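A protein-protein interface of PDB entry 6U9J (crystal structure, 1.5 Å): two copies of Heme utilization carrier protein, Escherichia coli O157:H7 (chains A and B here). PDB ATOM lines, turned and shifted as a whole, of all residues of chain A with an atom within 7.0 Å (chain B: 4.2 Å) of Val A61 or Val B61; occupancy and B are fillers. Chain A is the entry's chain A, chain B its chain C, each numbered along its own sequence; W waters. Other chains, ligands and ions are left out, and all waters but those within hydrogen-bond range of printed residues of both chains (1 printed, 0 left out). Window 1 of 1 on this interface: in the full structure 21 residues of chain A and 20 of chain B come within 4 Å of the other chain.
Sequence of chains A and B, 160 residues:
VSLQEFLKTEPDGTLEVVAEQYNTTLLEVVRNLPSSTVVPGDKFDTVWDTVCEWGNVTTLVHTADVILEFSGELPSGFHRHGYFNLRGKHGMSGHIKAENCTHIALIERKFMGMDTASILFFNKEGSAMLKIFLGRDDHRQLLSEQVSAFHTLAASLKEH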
ATOM      1  N   THR A  59      -5.982  33.474  -0.007  1.00  0.00           N
ATOM      2  CA  THR A  59      -7.028  32.786  -0.744  1.00  0.00           C
ATOM      3  C   THR A  59      -6.878  31.291  -0.516  1.00  0.00           C
ATOM      4  O   THR A  59      -5.773  30.756  -0.642  1.00  0.00           O
ATOM      5  CB  THR A  59      -6.931  33.101  -2.235  1.00  0.00           C
ATOM      6  OG1 THR A  59      -7.019  34.517  -2.427  1.00  0.00           O
ATOM      7  CG2 THR A  59      -8.050  32.411  -3.000  1.00  0.00           C
ATOM      8  N   LEU A  60      -7.972  30.633  -0.166  1.00  0.00           N
ATOM      9  CA  LEU A  60      -7.944  29.242   0.259  1.00  0.00           C
ATOM     10  C   LEU A  60      -8.940  28.420  -0.548  1.00  0.00           C
ATOM     11  O   LEU A  60     -10.077  28.844  -0.769  1.00  0.00           O
ATOM     12  CB  LEU A  60      -8.259  29.150   1.770  1.00  0.00           C
ATOM     13  CG  LEU A  60      -8.279  27.796   2.479  1.00  0.00           C
ATOM     14  CD1 LEU A  60      -7.781  27.940   3.914  1.00  0.00           C
ATOM     15  CD2 LEU A  60      -9.677  27.192   2.444  1.00  0.00           C
ATOM     16  N   VAL A  61      -8.517  27.234  -0.986  1.00  0.00           N
ATOM     17  CA  VAL A  61      -9.431  26.243  -1.533  1.00  0.00           C
ATOM     18  C   VAL A  61      -9.267  24.955  -0.736  1.00  0.00           C
ATOM     19  O   VAL A  61      -8.149  24.582  -0.365  1.00  0.00           O
ATOM     20  CB  VAL A  61      -9.198  26.016  -3.040  1.00  0.00           C
ATOM     21  CG1 VAL A  61      -7.812  25.449  -3.298  1.00  0.00           C
ATOM     22  CG2 VAL A  61     -10.292  25.118  -3.610  1.00  0.00           C
ATOM     23  N   HIS A  62     -10.388  24.289  -0.467  1.00  0.00           N
ATOM     24  CA  HIS A  62     -10.481  23.167   0.466  1.00  0.00           C
ATOM     25  C   HIS A  62     -11.128  21.998  -0.264  1.00  0.00           C
ATOM     26  O   HIS A  62     -12.295  22.086  -0.663  1.00  0.00           O
ATOM     27  CB  HIS A  62     -11.306  23.580   1.688  1.00  0.00           C
ATOM     28  CG  HIS A  62     -11.167  22.683   2.881  1.00  0.00           C
ATOM     29  ND1 HIS A  62     -11.656  23.031   4.121  1.00  0.00           N
ATOM     30  CD2 HIS A  62     -10.627  21.450   3.022  1.00  0.00           C
ATOM     31  CE1 HIS A  62     -11.406  22.060   4.981  1.00  0.00           C
ATOM     32  NE2 HIS A  62     -10.783  21.088   4.340  1.00  0.00           N
ATOM     33  N   THR A  63     -10.378  20.917  -0.468  1.00  0.00           N
ATOM     34  CA  THR A  63     -10.933  19.671  -0.976  1.00  0.00           C
ATOM     35  C   THR A  63     -10.872  18.619   0.125  1.00  0.00           C
ATOM     36  O   THR A  63     -10.436  18.886   1.250  1.00  0.00           O
ATOM     37  CB  THR A  63     -10.189  19.179  -2.221  1.00  0.00           C
ATOM     38  OG1 THR A  63      -8.950  18.571  -1.830  1.00  0.00           O
ATOM     39  CG2 THR A  63      -9.901  20.330  -3.164  1.00  0.00           C
ATOM     40  N   VAL A  66      -6.819  18.069   0.320  1.00  0.00           N
ATOM     41  CA  VAL A  66      -5.831  19.131   0.174  1.00  0.00           C
ATOM     42  C   VAL A  66      -6.459  20.446   0.621  1.00  0.00           C
ATOM     43  O   VAL A  66      -7.645  20.690   0.367  1.00  0.00           O
ATOM     44  CB  VAL A  66      -5.335  19.234  -1.290  1.00  0.00           C
ATOM     45  CG1 VAL A  66      -4.493  20.491  -1.514  1.00  0.00           C
ATOM     46  CG2 VAL A  66      -4.556  17.986  -1.696  1.00  0.00           C
ATOM     47  N   ILE A  67      -5.663  21.285   1.268  1.00  0.00           N
ATOM     48  CA  ILE A  67      -5.953  22.700   1.429  1.00  0.00           C
ATOM     49  C   ILE A  67      -4.747  23.430   0.873  1.00  0.00           C
ATOM     50  O   ILE A  67      -3.619  23.206   1.325  1.00  0.00           O
ATOM     51  CB  ILE A  67      -6.191  23.101   2.891  1.00  0.00           C
ATOM     52  CG1 ILE A  67      -7.453  22.431   3.438  1.00  0.00           C
ATOM     53  CG2 ILE A  67      -6.291  24.621   2.984  1.00  0.00           C
ATOM     54  CD1 ILE A  67      -8.012  23.111   4.680  1.00  0.00           C
ATOM     55  N   LEU A  68      -4.965  24.269  -0.121  1.00  0.00           N
ATOM     56  CA  LEU A  68      -3.910  25.131  -0.608  1.00  0.00           C
ATOM     57  C   LEU A  68      -4.295  26.563  -0.294  1.00  0.00           C
ATOM     58  O   LEU A  68      -5.460  26.948  -0.446  1.00  0.00           O
ATOM     59  CB  LEU A  68      -3.675  24.963  -2.110  1.00  0.00           C
ATOM     60  CG  LEU A  68      -2.926  23.694  -2.534  1.00  0.00           C
ATOM     61  CD1 LEU A  68      -2.400  23.866  -3.946  1.00  0.00           C
ATOM     62  CD2 LEU A  68      -1.794  23.365  -1.583  1.00  0.00           C
ATOM     63  N   GLU A  69      -3.333  27.332   0.175  1.00  0.00           N
ATOM     64  CA  GLU A  69      -3.598  28.727   0.468  1.00  0.00           C
ATOM     65  C   GLU A  69      -2.517  29.568  -0.163  1.00  0.00           C
ATOM     66  O   GLU A  69      -1.339  29.199  -0.166  1.00  0.00           O
ATOM     67  CB  GLU A  69      -3.689  29.013   1.965  1.00  0.00           C
ATOM     68  CG  GLU A  69      -2.671  28.344   2.824  1.00  0.00           C
ATOM     69  CD  GLU A  69      -3.126  28.284   4.278  1.00  0.00           C
ATOM     70  OE1 GLU A  69      -3.693  27.249   4.694  1.00  0.00           O
ATOM     71  OE2 GLU A  69      -2.939  29.286   5.002  1.00  0.00           O
ATOM     72  N   PHE A  70      -2.925  30.699  -0.708  1.00  0.00           N
ATOM     73  CA  PHE A  70      -2.011  31.608  -1.386  1.00  0.00           C
ATOM     74  C   PHE A  70      -2.073  32.961  -0.705  1.00  0.00           C
ATOM     75  O   PHE A  70      -3.141  33.574  -0.633  1.00  0.00           O
ATOM     76  CB  PHE A  70      -2.344  31.777  -2.866  1.00  0.00           C
ATOM     77  CG  PHE A  70      -1.512  32.839  -3.544  1.00  0.00           C
ATOM     78  CD1 PHE A  70      -0.223  32.560  -3.966  1.00  0.00           C
ATOM     79  CD2 PHE A  70      -2.017  34.115  -3.757  1.00  0.00           C
ATOM     80  CE1 PHE A  70       0.548  33.529  -4.585  1.00  0.00           C
ATOM     81  CE2 PHE A  70      -1.251  35.089  -4.378  1.00  0.00           C
ATOM     82  CZ  PHE A  70       0.032  34.793  -4.792  1.00  0.00           C
ATOM     83  N   ALA A 128     -18.934  25.925   0.549  1.00  0.00           N
ATOM     84  CA  ALA A 128     -17.962  26.914   0.112  1.00  0.00           C
ATOM     85  C   ALA A 128     -17.221  26.417  -1.125  1.00  0.00           C
ATOM     86  O   ALA A 128     -16.790  25.260  -1.180  1.00  0.00           O
ATOM     87  CB  ALA A 128     -16.976  27.219   1.248  1.00  0.00           C
ATOM     88  N   MET A 129     -17.101  27.282  -2.128  1.00  0.00           N
ATOM     89  CA  MET A 129     -16.220  26.999  -3.252  1.00  0.00           C
ATOM     90  C   MET A 129     -14.885  27.723  -3.154  1.00  0.00           C
ATOM     91  O   MET A 129     -13.921  27.305  -3.802  1.00  0.00           O
ATOM     92  CB  MET A 129     -16.898  27.338  -4.595  1.00  0.00           C
ATOM     93  CG  MET A 129     -17.917  28.458  -4.563  1.00  0.00           C
ATOM     94  SD  MET A 129     -18.636  28.776  -6.199  1.00  0.00           S
ATOM     95  CE  MET A 129     -17.152  29.363  -6.913  1.00  0.00           C
ATOM     96  N   LEU A 130     -14.782  28.746  -2.310  1.00  0.00           N
ATOM     97  CA  LEU A 130     -13.548  29.506  -2.203  1.00  0.00           C
ATOM     98  C   LEU A 130     -13.661  30.350  -0.950  1.00  0.00           C
ATOM     99  O   LEU A 130     -14.764  30.728  -0.565  1.00  0.00           O
ATOM    100  CB  LEU A 130     -13.333  30.398  -3.431  1.00  0.00           C
ATOM    101  CG  LEU A 130     -11.933  30.975  -3.574  1.00  0.00           C
ATOM    102  CD1 LEU A 130     -10.927  29.893  -3.951  1.00  0.00           C
ATOM    103  CD2 LEU A 130     -11.944  32.092  -4.604  1.00  0.00           C
ATOM    104  N   LYS A 131     -12.524  30.617  -0.303  1.00  0.00           N
ATOM    105  CA  LYS A 131     -12.481  31.509   0.849  1.00  0.00           C
ATOM    106  C   LYS A 131     -11.337  32.495   0.684  1.00  0.00           C
ATOM    107  O   LYS A 131     -10.279  32.147   0.155  1.00  0.00           O
ATOM    108  CB  LYS A 131     -12.290  30.727   2.171  1.00  0.00           C
ATOM    109  CG  LYS A 131     -13.407  29.737   2.486  1.00  0.00           C
ATOM    110  CD  LYS A 131     -13.251  29.148   3.885  1.00  0.00           C
ATOM    111  CE  LYS A 131     -14.324  28.114   4.176  1.00  0.00           C
ATOM    112  NZ  LYS A 131     -14.239  27.662   5.607  1.00  0.00           N
ATOM    113  N   LEU B  60      -1.413  22.559  -9.158  1.00  0.00           N
ATOM    114  CA  LEU B  60      -2.804  22.759  -9.545  1.00  0.00           C
ATOM    115  C   LEU B  60      -3.738  21.933  -8.666  1.00  0.00           C
ATOM    116  O   LEU B  60      -3.476  20.752  -8.421  1.00  0.00           O
ATOM    117  CB  LEU B  60      -2.981  22.385 -11.036  1.00  0.00           C
ATOM    118  CG  LEU B  60      -4.361  22.513 -11.672  1.00  0.00           C
ATOM    119  CD1 LEU B  60      -4.214  22.900 -13.141  1.00  0.00           C
ATOM    120  CD2 LEU B  60      -5.173  21.231 -11.515  1.00  0.00           C
ATOM    121  N   VAL B  61      -4.833  22.550  -8.201  1.00  0.00           N
ATOM    122  CA  VAL B  61      -5.928  21.854  -7.535  1.00  0.00           C
ATOM    123  C   VAL B  61      -7.207  22.091  -8.335  1.00  0.00           C
ATOM    124  O   VAL B  61      -7.485  23.224  -8.727  1.00  0.00           O
ATOM    125  CB  VAL B  61      -6.112  22.338  -6.083  1.00  0.00           C
ATOM    126  CG1 VAL B  61      -5.219  21.557  -5.158  1.00  0.00           C
ATOM    127  CG2 VAL B  61      -5.833  23.824  -5.984  1.00  0.00           C
ATOM    128  N   HIS B  62      -7.977  21.021  -8.531  1.00  0.00           N
ATOM    129  CA  HIS B  62      -9.202  20.996  -9.329  1.00  0.00           C
ATOM    130  C   HIS B  62     -10.363  20.638  -8.410  1.00  0.00           C
ATOM    131  O   HIS B  62     -10.362  19.561  -7.802  1.00  0.00           O
ATOM    132  CB  HIS B  62      -9.066  19.954 -10.449  1.00  0.00           C
ATOM    133  CG  HIS B  62     -10.090  20.057 -11.540  1.00  0.00           C
ATOM    134  ND1 HIS B  62     -11.426  20.296 -11.300  1.00  0.00           N
ATOM    135  CD2 HIS B  62      -9.969  19.919 -12.883  1.00  0.00           C
ATOM    136  CE1 HIS B  62     -12.081  20.323 -12.447  1.00  0.00           C
ATOM    137  NE2 HIS B  62     -11.220  20.099 -13.424  1.00  0.00           N
ATOM    138  N   THR B  63     -11.339  21.535  -8.287  1.00  0.00           N
ATOM    139  CA  THR B  63     -12.618  21.209  -7.662  1.00  0.00           C
ATOM    140  C   THR B  63     -13.724  21.362  -8.700  1.00  0.00           C
ATOM    141  O   THR B  63     -13.472  21.683  -9.866  1.00  0.00           O
ATOM    142  CB  THR B  63     -12.917  22.091  -6.447  1.00  0.00           C
ATOM    143  OG1 THR B  63     -13.331  23.391  -6.887  1.00  0.00           O
ATOM    144  CG2 THR B  63     -11.692  22.230  -5.562  1.00  0.00           C
ATOM    145  N   VAL B  66     -13.671  25.422  -9.150  1.00  0.00           N
ATOM    146  CA  VAL B  66     -12.480  26.255  -9.073  1.00  0.00           C
ATOM    147  C   VAL B  66     -11.293  25.442  -9.571  1.00  0.00           C
ATOM    148  O   VAL B  66     -11.180  24.247  -9.274  1.00  0.00           O
ATOM    149  CB  VAL B  66     -12.233  26.748  -7.624  1.00  0.00           C
ATOM    150  CG1 VAL B  66     -10.850  27.379  -7.474  1.00  0.00           C
ATOM    151  CG2 VAL B  66     -13.328  27.720  -7.185  1.00  0.00           C
ATOM    152  N   ILE B  67     -10.420  26.088 -10.339  1.00  0.00           N
ATOM    153  CA  ILE B  67      -9.051  25.631 -10.545  1.00  0.00           C
ATOM    154  C   ILE B  67      -8.144  26.728 -10.034  1.00  0.00           C
ATOM    155  O   ILE B  67      -8.234  27.873 -10.483  1.00  0.00           O
ATOM    156  CB  ILE B  67      -8.727  25.351 -12.017  1.00  0.00           C
ATOM    157  CG1 ILE B  67      -9.812  24.500 -12.657  1.00  0.00           C
ATOM    158  CG2 ILE B  67      -7.360  24.697 -12.107  1.00  0.00           C
ATOM    159  CD1 ILE B  67      -9.807  23.137 -12.177  1.00  0.00           C
ATOM    160  N   LEU B  68      -7.278  26.395  -9.099  1.00  0.00           N
ATOM    161  CA  LEU B  68      -6.258  27.332  -8.673  1.00  0.00           C
ATOM    162  C   LEU B  68      -4.920  26.741  -9.066  1.00  0.00           C
ATOM    163  O   LEU B  68      -4.699  25.536  -8.903  1.00  0.00           O
ATOM    164  CB  LEU B  68      -6.313  27.604  -7.168  1.00  0.00           C
ATOM    165  CG  LEU B  68      -7.484  28.486  -6.719  1.00  0.00           C
ATOM    166  CD1 LEU B  68      -7.334  28.893  -5.261  1.00  0.00           C
ATOM    167  CD2 LEU B  68      -7.626  29.711  -7.606  1.00  0.00           C
ATOM    168  N   LEU B 130      -4.082  16.206  -6.570  1.00  0.00           N
ATOM    169  CA  LEU B 130      -3.157  17.308  -6.787  1.00  0.00           C
ATOM    170  C   LEU B 130      -2.416  17.018  -8.079  1.00  0.00           C
ATOM    171  O   LEU B 130      -2.217  15.857  -8.420  1.00  0.00           O
ATOM    172  CB  LEU B 130      -2.168  17.440  -5.625  1.00  0.00           C
ATOM    173  CG  LEU B 130      -1.326  18.700  -5.613  1.00  0.00           C
ATOM    174  CD1 LEU B 130      -2.164  19.889  -5.237  1.00  0.00           C
ATOM    175  CD2 LEU B 130      -0.189  18.542  -4.624  1.00  0.00           C
HETATM  176  O   HOH W   1     -14.155  24.699  -4.785  1.00  0.00           O
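N of Val A61 lies within hydrogen-bond range of O of Leu A68, 3.1 Å away. N of Val B61 sits at hydrogen-bond distance from O of Leu B68 (3.1 Å). N of Val A66 sits at hydrogen-bond distance from OG1 of Thr A63 (3.1 Å). The side-chain hydroxyl (OG1) of Thr B63 sits at hydrogen-bond distance from the backbone NH (N) of Val B66 (3.1 Å).
CG2 of Val B61 touches CG1 of Val A61, at 3.7 Å. CG2 of Val A61 touches CG2 of Thr B63, at 3.8 Å. CG1 of Val A61 touches CD1 of Leu B68, at 3.99 Å. Thr B63 touches Thr A63 (CG2 to CG2, 3.5 Å). Val A66 touches Val B61 (CG1 to CG1, 3.9 Å). Val B61 touches Leu A68. Met A129 touches Val B66. Leu B68 touches Leu A130.
Printed residues of chain B within 4 Å of Val A61: Val B61, Thr B63 and Leu B68. Of the printed residues of chain A, Val B61 touches Val A61 (3.7 Å), Val A66 (3.9 Å) and Leu A68 (3.8 Å). Of the printed residues of chain B, Thr A63 touches Thr B63. Of the printed residues of chain B, Leu A68 touches Val B61. Of the printed residues of chain A, Val B66 touches Met A129 (3.5 Å).
Hydrophobic or aromatic side chains of chain A that line the printed part of chain B: Val A61, Val A66, Leu A68 and Leu A130. Among the printed residues, no Asp or Glu carboxylate lies within 4 Å of a Lys or Arg side-chain nitrogen of the other chain.
Val B61 touches its own counterpart, Val A61. Val A61 touches Leu B68, and with the chains exchanged Leu A68 touches Val B61. Val A66 touches Val B61, but with the chains exchanged Val A61 does not touch Val B66 (4.5 Å). Leu A130 touches Leu B68, but with the chains exchanged Leu A68 does not touch Leu B130 (4.2 Å). Of the 8 pairs that touch across the chains among the printed residues, 4 have their exchanged pair printed and touching as well.
Water W1 bridges the side-chain hydroxyl of Thr B63 (2.6 Å) and the backbone carbonyl oxygen of Met A129 (2.8 Å).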
